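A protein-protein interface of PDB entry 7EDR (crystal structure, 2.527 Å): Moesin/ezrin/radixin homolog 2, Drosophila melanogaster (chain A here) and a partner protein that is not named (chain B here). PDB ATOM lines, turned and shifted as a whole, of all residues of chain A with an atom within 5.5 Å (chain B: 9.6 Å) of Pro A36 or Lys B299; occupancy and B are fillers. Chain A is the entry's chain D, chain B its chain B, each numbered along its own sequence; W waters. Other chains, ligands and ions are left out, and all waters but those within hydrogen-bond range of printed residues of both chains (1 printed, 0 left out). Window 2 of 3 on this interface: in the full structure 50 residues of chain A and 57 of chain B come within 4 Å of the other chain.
The side-chain hydroxyl (OG1) of Thr B302 lies within hydrogen-bond range of the backbone carbonyl oxygen (O) of Lys B299, at 3.0 Å. The side-chain carboxylate (OE2) of Glu B90 is in salt-bridge range of the guanidinium group (NH1) of Arg B298 (2.8 Å). The side-chain carboxylate (OE2) of Glu A35 lies within hydrogen-bond range of the backbone NH (N) of Lys A37 (3.1 Å). O of Arg B296 lies within hydrogen-bond range of OG1 of Thr B302 (2.9 Å). O of Tyr B294 is in hydrogen-bond range of NH1 of Arg B298, at 2.9 Å.
Water W1 bridges the backbone NH of Glu A35 (2.7 Å) and the backbone carbonyl oxygen of Asp B301 (3.3 Å).
Glu A35 touches just these residues of chain B: Asp B301 and Thr B302. Pro A36 touches just these residues of chain B: Lys B299 (3.8 Å) and Thr B302 (3.7 Å). Of the printed residues of chain B, Leu A41 touches Arg B298. Leu B293 touches none of the printed residues of chain A. Of the printed residues of chain A, Met B295 touches Phe A39. Printed residues of chain A within 4 Å of Arg B296: Phe A34. Of the printed residues of chain A, Arg B298 touches Leu A41 (3.7 Å). Of chain A, only Pro A36 (3.8 Å) and Phe A39 (3.4 Å) come within 4 Å of Lys B299. Printed residues of chain A within 4 Å of Asp B301: Glu A35. The nearest residue of chain B that does not touch Pro A36 is Asp B301 (4.2 Å). The nearest residue of chain A that does not touch Lys B299 is Leu A41 (4.9 Å).
The backbone carbonyl oxygen (O) of Glu A35 sits close to the backbone carbonyl oxygen (O) of Asp B301 (3.4 Å).
Of the 8 printed residues of chain A, 5 touch a printed residue of chain B. Printed residues of chain A that touch a printed residue of chain B: Phe A34, Glu A35, Pro A36, Phe A39 and Leu A41. Hydrophobic or aromatic side chains of chain A that line the printed part of chain B: Phe A34, Pro A36, Phe A39 and Leu A41. Of the 15 printed residues of chain B, 6 touch a printed residue of chain A. Among the printed residues, 9 pairs touch across the chains.
Among the printed residues, pairs that only touch across the chains: Phe A34 with Arg B296, Phe A34 with Thr B302, Phe A39 with Lys B299, Glu A35 with Thr B302, Leu A41 with Arg B298, Phe A39 with Met B295, Pro A36 with Thr B302 and Pro A36 with Lys B299.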
ATOM      1  N   PHE A  34     -15.534  32.346  10.694  1.00  0.00           N
ATOM      2  CA  PHE A  34     -15.820  31.119   9.974  1.00  0.00           C
ATOM      3  C   PHE A  34     -16.385  31.463   8.601  1.00  0.00           C
ATOM      4  O   PHE A  34     -16.689  32.622   8.295  1.00  0.00           O
ATOM      5  CB  PHE A  34     -16.812  30.260  10.774  1.00  0.00           C
ATOM      6  CG  PHE A  34     -18.108  30.973  11.096  1.00  0.00           C
ATOM      7  CD1 PHE A  34     -19.207  30.878  10.238  1.00  0.00           C
ATOM      8  CD2 PHE A  34     -18.218  31.768  12.229  1.00  0.00           C
ATOM      9  CE1 PHE A  34     -20.394  31.548  10.526  1.00  0.00           C
ATOM     10  CE2 PHE A  34     -19.403  32.437  12.525  1.00  0.00           C
ATOM     11  CZ  PHE A  34     -20.488  32.333  11.683  1.00  0.00           C
ATOM     12  N   GLU A  35     -16.545  30.434   7.775  1.00  0.00           N
ATOM     13  CA  GLU A  35     -17.148  30.607   6.454  1.00  0.00           C
ATOM     14  C   GLU A  35     -18.016  29.396   6.083  1.00  0.00           C
ATOM     15  O   GLU A  35     -17.680  28.272   6.414  1.00  0.00           O
ATOM     16  CB  GLU A  35     -16.054  30.846   5.404  1.00  0.00           C
ATOM     17  CG  GLU A  35     -15.786  32.325   5.116  1.00  0.00           C
ATOM     18  CD  GLU A  35     -16.906  32.992   4.292  1.00  0.00           C
ATOM     19  OE1 GLU A  35     -17.200  32.503   3.171  1.00  0.00           O
ATOM     20  OE2 GLU A  35     -17.492  34.006   4.759  1.00  0.00           O
ATOM     21  N   PRO A  36     -19.151  29.620   5.404  1.00  0.00           N
ATOM     22  CA  PRO A  36     -19.692  30.906   4.953  1.00  0.00           C
ATOM     23  C   PRO A  36     -20.315  31.720   6.096  1.00  0.00           C
ATOM     24  O   PRO A  36     -20.903  31.150   7.010  1.00  0.00           O
ATOM     25  CB  PRO A  36     -20.755  30.494   3.931  1.00  0.00           C
ATOM     26  CG  PRO A  36     -21.221  29.143   4.393  1.00  0.00           C
ATOM     27  CD  PRO A  36     -20.059  28.494   5.095  1.00  0.00           C
ATOM     28  N   LYS A  37     -20.171  33.044   6.051  1.00  0.00           N
ATOM     29  CA  LYS A  37     -20.744  33.869   7.104  1.00  0.00           C
ATOM     30  C   LYS A  37     -22.246  34.036   6.913  1.00  0.00           C
ATOM     31  O   LYS A  37     -22.975  34.234   7.894  1.00  0.00           O
ATOM     32  CB  LYS A  37     -20.034  35.224   7.143  1.00  0.00           C
ATOM     33  CG  LYS A  37     -19.773  35.763   8.540  1.00  0.00           C
ATOM     34  CD  LYS A  37     -18.938  34.785   9.365  1.00  0.00           C
ATOM     35  CE  LYS A  37     -18.558  35.365  10.729  1.00  0.00           C
ATOM     36  NZ  LYS A  37     -17.568  36.470  10.600  1.00  0.00           N
ATOM     37  N   GLU A  38     -22.723  33.941   5.670  1.00  0.00           N
ATOM     38  CA  GLU A  38     -24.142  33.965   5.347  1.00  0.00           C
ATOM     39  C   GLU A  38     -24.495  32.657   4.661  1.00  0.00           C
ATOM     40  O   GLU A  38     -23.770  32.215   3.759  1.00  0.00           O
ATOM     41  CB  GLU A  38     -24.503  35.151   4.443  1.00  0.00           C
ATOM     42  CG  GLU A  38     -24.016  36.509   4.967  1.00  0.00           C
ATOM     43  CD  GLU A  38     -24.363  37.707   4.057  1.00  0.00           C
ATOM     44  OE1 GLU A  38     -24.399  37.542   2.805  1.00  0.00           O
ATOM     45  OE2 GLU A  38     -24.586  38.817   4.607  1.00  0.00           O
ATOM     46  N   PHE A  39     -25.593  32.031   5.096  1.00  0.00           N
ATOM     47  CA  PHE A  39     -26.066  30.811   4.447  1.00  0.00           C
ATOM     48  C   PHE A  39     -27.561  30.642   4.715  1.00  0.00           C
ATOM     49  O   PHE A  39     -28.155  31.302   5.570  1.00  0.00           O
ATOM     50  CB  PHE A  39     -25.255  29.561   4.880  1.00  0.00           C
ATOM     51  CG  PHE A  39     -25.254  29.308   6.373  1.00  0.00           C
ATOM     52  CD1 PHE A  39     -24.346  29.957   7.209  1.00  0.00           C
ATOM     53  CD2 PHE A  39     -26.176  28.428   6.947  1.00  0.00           C
ATOM     54  CE1 PHE A  39     -24.346  29.738   8.592  1.00  0.00           C
ATOM     55  CE2 PHE A  39     -26.183  28.196   8.331  1.00  0.00           C
ATOM     56  CZ  PHE A  39     -25.259  28.858   9.153  1.00  0.00           C
ATOM     57  N   ILE A  40     -28.162  29.746   3.957  1.00  0.00           N
ATOM     58  CA  ILE A  40     -29.593  29.530   4.005  1.00  0.00           C
ATOM     59  C   ILE A  40     -29.831  28.045   4.225  1.00  0.00           C
ATOM     60  O   ILE A  40     -29.276  27.205   3.502  1.00  0.00           O
ATOM     61  CB  ILE A  40     -30.287  30.028   2.724  1.00  0.00           C
ATOM     62  CG1 ILE A  40     -30.194  31.550   2.657  1.00  0.00           C
ATOM     63  CG2 ILE A  40     -31.740  29.559   2.700  1.00  0.00           C
ATOM     64  CD1 ILE A  40     -30.643  32.173   1.342  1.00  0.00           C
ATOM     65  N   LEU A  41     -30.625  27.723   5.242  1.00  0.00           N
ATOM     66  CA  LEU A  41     -30.992  26.346   5.542  1.00  0.00           C
ATOM     67  C   LEU A  41     -32.459  26.168   5.219  1.00  0.00           C
ATOM     68  O   LEU A  41     -33.330  26.803   5.821  1.00  0.00           O
ATOM     69  CB  LEU A  41     -30.725  25.977   6.994  1.00  0.00           C
ATOM     70  CG  LEU A  41     -29.252  25.767   7.302  1.00  0.00           C
ATOM     71  CD1 LEU A  41     -29.089  25.842   8.790  1.00  0.00           C
ATOM     72  CD2 LEU A  41     -28.809  24.434   6.786  1.00  0.00           C
ATOM     73  N   TRP B  43     -14.891  27.814  19.736  1.00  0.00           N
ATOM     74  CA  TRP B  43     -16.228  28.382  19.870  1.00  0.00           C
ATOM     75  C   TRP B  43     -16.958  27.913  21.132  1.00  0.00           C
ATOM     76  O   TRP B  43     -17.854  28.620  21.615  1.00  0.00           O
ATOM     77  CB  TRP B  43     -17.052  28.049  18.625  1.00  0.00           C
ATOM     78  CG  TRP B  43     -16.693  26.759  17.954  1.00  0.00           C
ATOM     79  CD1 TRP B  43     -17.135  25.512  18.286  1.00  0.00           C
ATOM     80  CD2 TRP B  43     -15.840  26.594  16.817  1.00  0.00           C
ATOM     81  NE1 TRP B  43     -16.602  24.579  17.430  1.00  0.00           N
ATOM     82  CE2 TRP B  43     -15.804  25.217  16.518  1.00  0.00           C
ATOM     83  CE3 TRP B  43     -15.116  27.480  16.013  1.00  0.00           C
ATOM     84  CZ2 TRP B  43     -15.061  24.700  15.454  1.00  0.00           C
ATOM     85  CZ3 TRP B  43     -14.366  26.964  14.957  1.00  0.00           C
ATOM     86  CH2 TRP B  43     -14.345  25.585  14.691  1.00  0.00           C
ATOM     87  N   GLU B  90     -24.147  19.124  20.616  1.00  0.00           N
ATOM     88  CA  GLU B  90     -25.353  18.311  20.747  1.00  0.00           C
ATOM     89  C   GLU B  90     -25.033  16.825  20.735  1.00  0.00           C
ATOM     90  O   GLU B  90     -25.727  16.050  21.393  1.00  0.00           O
ATOM     91  CB  GLU B  90     -26.358  18.649  19.651  1.00  0.00           C
ATOM     92  CG  GLU B  90     -26.970  20.021  19.782  1.00  0.00           C
ATOM     93  CD  GLU B  90     -27.933  20.334  18.639  1.00  0.00           C
ATOM     94  OE1 GLU B  90     -28.758  19.443  18.313  1.00  0.00           O
ATOM     95  OE2 GLU B  90     -27.874  21.458  18.068  1.00  0.00           O
ATOM     96  N   ASP B 292     -26.361  30.791  17.882  1.00  0.00           N
ATOM     97  CA  ASP B 292     -25.321  30.830  16.853  1.00  0.00           C
ATOM     98  C   ASP B 292     -24.822  29.433  16.517  1.00  0.00           C
ATOM     99  O   ASP B 292     -24.711  29.069  15.340  1.00  0.00           O
ATOM    100  CB  ASP B 292     -24.124  31.677  17.297  1.00  0.00           C
ATOM    101  CG  ASP B 292     -24.393  33.179  17.278  1.00  0.00           C
ATOM    102  OD1 ASP B 292     -25.299  33.652  16.552  1.00  0.00           O
ATOM    103  OD2 ASP B 292     -23.657  33.898  17.998  1.00  0.00           O
ATOM    104  N   LEU B 293     -24.482  28.643  17.542  1.00  0.00           N
ATOM    105  CA  LEU B 293     -23.894  27.338  17.269  1.00  0.00           C
ATOM    106  C   LEU B 293     -24.938  26.374  16.766  1.00  0.00           C
ATOM    107  O   LEU B 293     -24.613  25.472  15.989  1.00  0.00           O
ATOM    108  CB  LEU B 293     -23.214  26.753  18.508  1.00  0.00           C
ATOM    109  CG  LEU B 293     -21.969  27.517  18.919  1.00  0.00           C
ATOM    110  CD1 LEU B 293     -21.451  27.051  20.247  1.00  0.00           C
ATOM    111  CD2 LEU B 293     -20.919  27.325  17.866  1.00  0.00           C
ATOM    112  N   TYR B 294     -26.188  26.549  17.207  1.00  0.00           N
ATOM    113  CA  TYR B 294     -27.271  25.701  16.726  1.00  0.00           C
ATOM    114  C   TYR B 294     -27.355  25.738  15.198  1.00  0.00           C
ATOM    115  O   TYR B 294     -27.461  24.690  14.546  1.00  0.00           O
ATOM    116  CB  TYR B 294     -28.596  26.139  17.368  1.00  0.00           C
ATOM    117  CG  TYR B 294     -29.770  25.258  17.022  1.00  0.00           C
ATOM    118  CD1 TYR B 294     -30.546  25.501  15.885  1.00  0.00           C
ATOM    119  CD2 TYR B 294     -30.096  24.160  17.824  1.00  0.00           C
ATOM    120  CE1 TYR B 294     -31.624  24.680  15.557  1.00  0.00           C
ATOM    121  CE2 TYR B 294     -31.168  23.332  17.510  1.00  0.00           C
ATOM    122  CZ  TYR B 294     -31.932  23.592  16.377  1.00  0.00           C
ATOM    123  OH  TYR B 294     -32.997  22.758  16.077  1.00  0.00           O
ATOM    124  N   MET B 295     -27.289  26.939  14.612  1.00  0.00           N
ATOM    125  CA  MET B 295     -27.320  27.072  13.159  1.00  0.00           C
ATOM    126  C   MET B 295     -26.000  26.657  12.520  1.00  0.00           C
ATOM    127  O   MET B 295     -26.004  26.026  11.460  1.00  0.00           O
ATOM    128  CB  MET B 295     -27.660  28.505  12.767  1.00  0.00           C
ATOM    129  CG  MET B 295     -29.022  28.971  13.235  1.00  0.00           C
ATOM    130  SD  MET B 295     -30.364  28.015  12.491  1.00  0.00           S
ATOM    131  CE  MET B 295     -31.746  29.020  13.049  1.00  0.00           C
ATOM    132  N   ARG B 296     -24.868  27.019  13.136  1.00  0.00           N
ATOM    133  CA  ARG B 296     -23.567  26.682  12.565  1.00  0.00           C
ATOM    134  C   ARG B 296     -23.346  25.172  12.547  1.00  0.00           C
ATOM    135  O   ARG B 296     -22.815  24.623  11.576  1.00  0.00           O
ATOM    136  CB  ARG B 296     -22.449  27.379  13.349  1.00  0.00           C
ATOM    137  CG  ARG B 296     -22.375  28.885  13.124  1.00  0.00           C
ATOM    138  CD  ARG B 296     -21.300  29.495  13.982  1.00  0.00           C
ATOM    139  NE  ARG B 296     -19.991  28.886  13.701  1.00  0.00           N
ATOM    140  CZ  ARG B 296     -18.854  29.238  14.296  1.00  0.00           C
ATOM    141  NH1 ARG B 296     -18.858  30.194  15.211  1.00  0.00           N
ATOM    142  NH2 ARG B 296     -17.718  28.625  13.976  1.00  0.00           N
ATOM    143  N   ARG B 297     -23.748  24.492  13.618  1.00  0.00           N
ATOM    144  CA  ARG B 297     -23.686  23.036  13.684  1.00  0.00           C
ATOM    145  C   ARG B 297     -24.367  22.390  12.474  1.00  0.00           C
ATOM    146  O   ARG B 297     -23.916  21.353  11.968  1.00  0.00           O
ATOM    147  CB  ARG B 297     -24.345  22.598  15.005  1.00  0.00           C
ATOM    148  CG  ARG B 297     -24.436  21.146  15.314  1.00  0.00           C
ATOM    149  CD  ARG B 297     -24.942  20.982  16.760  1.00  0.00           C
ATOM    150  NE  ARG B 297     -24.024  21.635  17.682  1.00  0.00           N
ATOM    151  CZ  ARG B 297     -24.329  22.622  18.519  1.00  0.00           C
ATOM    152  NH1 ARG B 297     -25.569  23.089  18.616  1.00  0.00           N
ATOM    153  NH2 ARG B 297     -23.371  23.136  19.285  1.00  0.00           N
ATOM    154  N   ARG B 298     -25.457  22.989  11.995  1.00  0.00           N
ATOM    155  CA  ARG B 298     -26.210  22.445  10.867  1.00  0.00           C
ATOM    156  C   ARG B 298     -25.680  22.887   9.507  1.00  0.00           C
ATOM    157  O   ARG B 298     -26.236  22.476   8.484  1.00  0.00           O
ATOM    158  CB  ARG B 298     -27.690  22.807  11.016  1.00  0.00           C
ATOM    159  CG  ARG B 298     -28.196  22.242  12.292  1.00  0.00           C
ATOM    160  CD  ARG B 298     -29.525  22.725  12.771  1.00  0.00           C
ATOM    161  NE  ARG B 298     -30.081  21.714  13.668  1.00  0.00           N
ATOM    162  CZ  ARG B 298     -29.654  21.486  14.912  1.00  0.00           C
ATOM    163  NH1 ARG B 298     -28.660  22.211  15.437  1.00  0.00           N
ATOM    164  NH2 ARG B 298     -30.221  20.529  15.647  1.00  0.00           N
ATOM    165  N   LYS B 299     -24.619  23.692   9.472  1.00  0.00           N
ATOM    166  CA  LYS B 299     -23.894  24.030   8.247  1.00  0.00           C
ATOM    167  C   LYS B 299     -22.432  23.672   8.509  1.00  0.00           C
ATOM    168  O   LYS B 299     -21.594  24.551   8.757  1.00  0.00           O
ATOM    169  CB  LYS B 299     -24.094  25.508   7.885  1.00  0.00           C
ATOM    170  CG  LYS B 299     -23.441  25.987   6.583  1.00  0.00           C
ATOM    171  CD  LYS B 299     -24.224  25.567   5.350  1.00  0.00           C
ATOM    172  CE  LYS B 299     -23.678  26.259   4.100  1.00  0.00           C
ATOM    173  NZ  LYS B 299     -24.339  25.774   2.867  1.00  0.00           N
ATOM    174  N   PRO B 300     -22.090  22.366   8.464  1.00  0.00           N
ATOM    175  CA  PRO B 300     -20.798  21.897   9.007  1.00  0.00           C
ATOM    176  C   PRO B 300     -19.533  22.587   8.489  1.00  0.00           C
ATOM    177  O   PRO B 300     -18.506  22.574   9.186  1.00  0.00           O
ATOM    178  CB  PRO B 300     -20.804  20.408   8.643  1.00  0.00           C
ATOM    179  CG  PRO B 300     -22.262  20.029   8.701  1.00  0.00           C
ATOM    180  CD  PRO B 300     -22.990  21.241   8.128  1.00  0.00           C
ATOM    181  N   ASP B 301     -19.570  23.214   7.308  1.00  0.00           N
ATOM    182  CA  ASP B 301     -18.387  23.957   6.865  1.00  0.00           C
ATOM    183  C   ASP B 301     -18.002  25.069   7.842  1.00  0.00           C
ATOM    184  O   ASP B 301     -16.815  25.377   7.991  1.00  0.00           O
ATOM    185  CB  ASP B 301     -18.613  24.534   5.469  1.00  0.00           C
ATOM    186  CG  ASP B 301     -18.587  23.467   4.397  1.00  0.00           C
ATOM    187  OD1 ASP B 301     -18.079  22.364   4.683  1.00  0.00           O
ATOM    188  OD2 ASP B 301     -19.087  23.716   3.278  1.00  0.00           O
ATOM    189  N   THR B 302     -18.979  25.686   8.510  1.00  0.00           N
ATOM    190  CA  THR B 302     -18.675  26.720   9.491  1.00  0.00           C
ATOM    191  C   THR B 302     -17.910  26.184  10.696  1.00  0.00           C
ATOM    192  O   THR B 302     -17.414  26.992  11.492  1.00  0.00           O
ATOM    193  CB  THR B 302     -19.971  27.405   9.965  1.00  0.00           C
ATOM    194  OG1 THR B 302     -20.730  26.509  10.800  1.00  0.00           O
ATOM    195  CG2 THR B 302     -20.825  27.841   8.771  1.00  0.00           C
ATOM    196  N   MET B 303     -17.813  24.858  10.857  1.00  0.00           N
ATOM    197  CA  MET B 303     -17.120  24.250  11.992  1.00  0.00           C
ATOM    198  C   MET B 303     -15.795  23.617  11.602  1.00  0.00           C
ATOM    199  O   MET B 303     -15.220  22.875  12.405  1.00  0.00           O
ATOM    200  CB  MET B 303     -17.992  23.190  12.681  1.00  0.00           C
ATOM    201  CG  MET B 303     -19.394  23.657  13.062  1.00  0.00           C
ATOM    202  SD  MET B 303     -19.372  25.032  14.220  1.00  0.00           S
ATOM    203  CE  MET B 303     -20.168  24.259  15.630  1.00  0.00           C
ATOM    204  N   GLU B 304     -15.311  23.870  10.391  1.00  0.00           N
ATOM    205  CA  GLU B 304     -14.022  23.340   9.969  1.00  0.00           C
ATOM    206  C   GLU B 304     -12.886  23.942  10.775  1.00  0.00           C
ATOM    207  O   GLU B 304     -12.902  25.117  11.139  1.00  0.00           O
ATOM    208  CB  GLU B 304     -13.762  23.648   8.502  1.00  0.00           C
ATOM    209  CG  GLU B 304     -14.274  22.619   7.540  1.00  0.00           C
ATOM    210  CD  GLU B 304     -14.410  23.210   6.152  1.00  0.00           C
ATOM    211  OE1 GLU B 304     -15.380  22.848   5.448  1.00  0.00           O
ATOM    212  OE2 GLU B 304     -13.565  24.064   5.780  1.00  0.00           O
HETATM  213  O   HOH W   1     -15.145  28.159   8.210  1.00  0.00           O
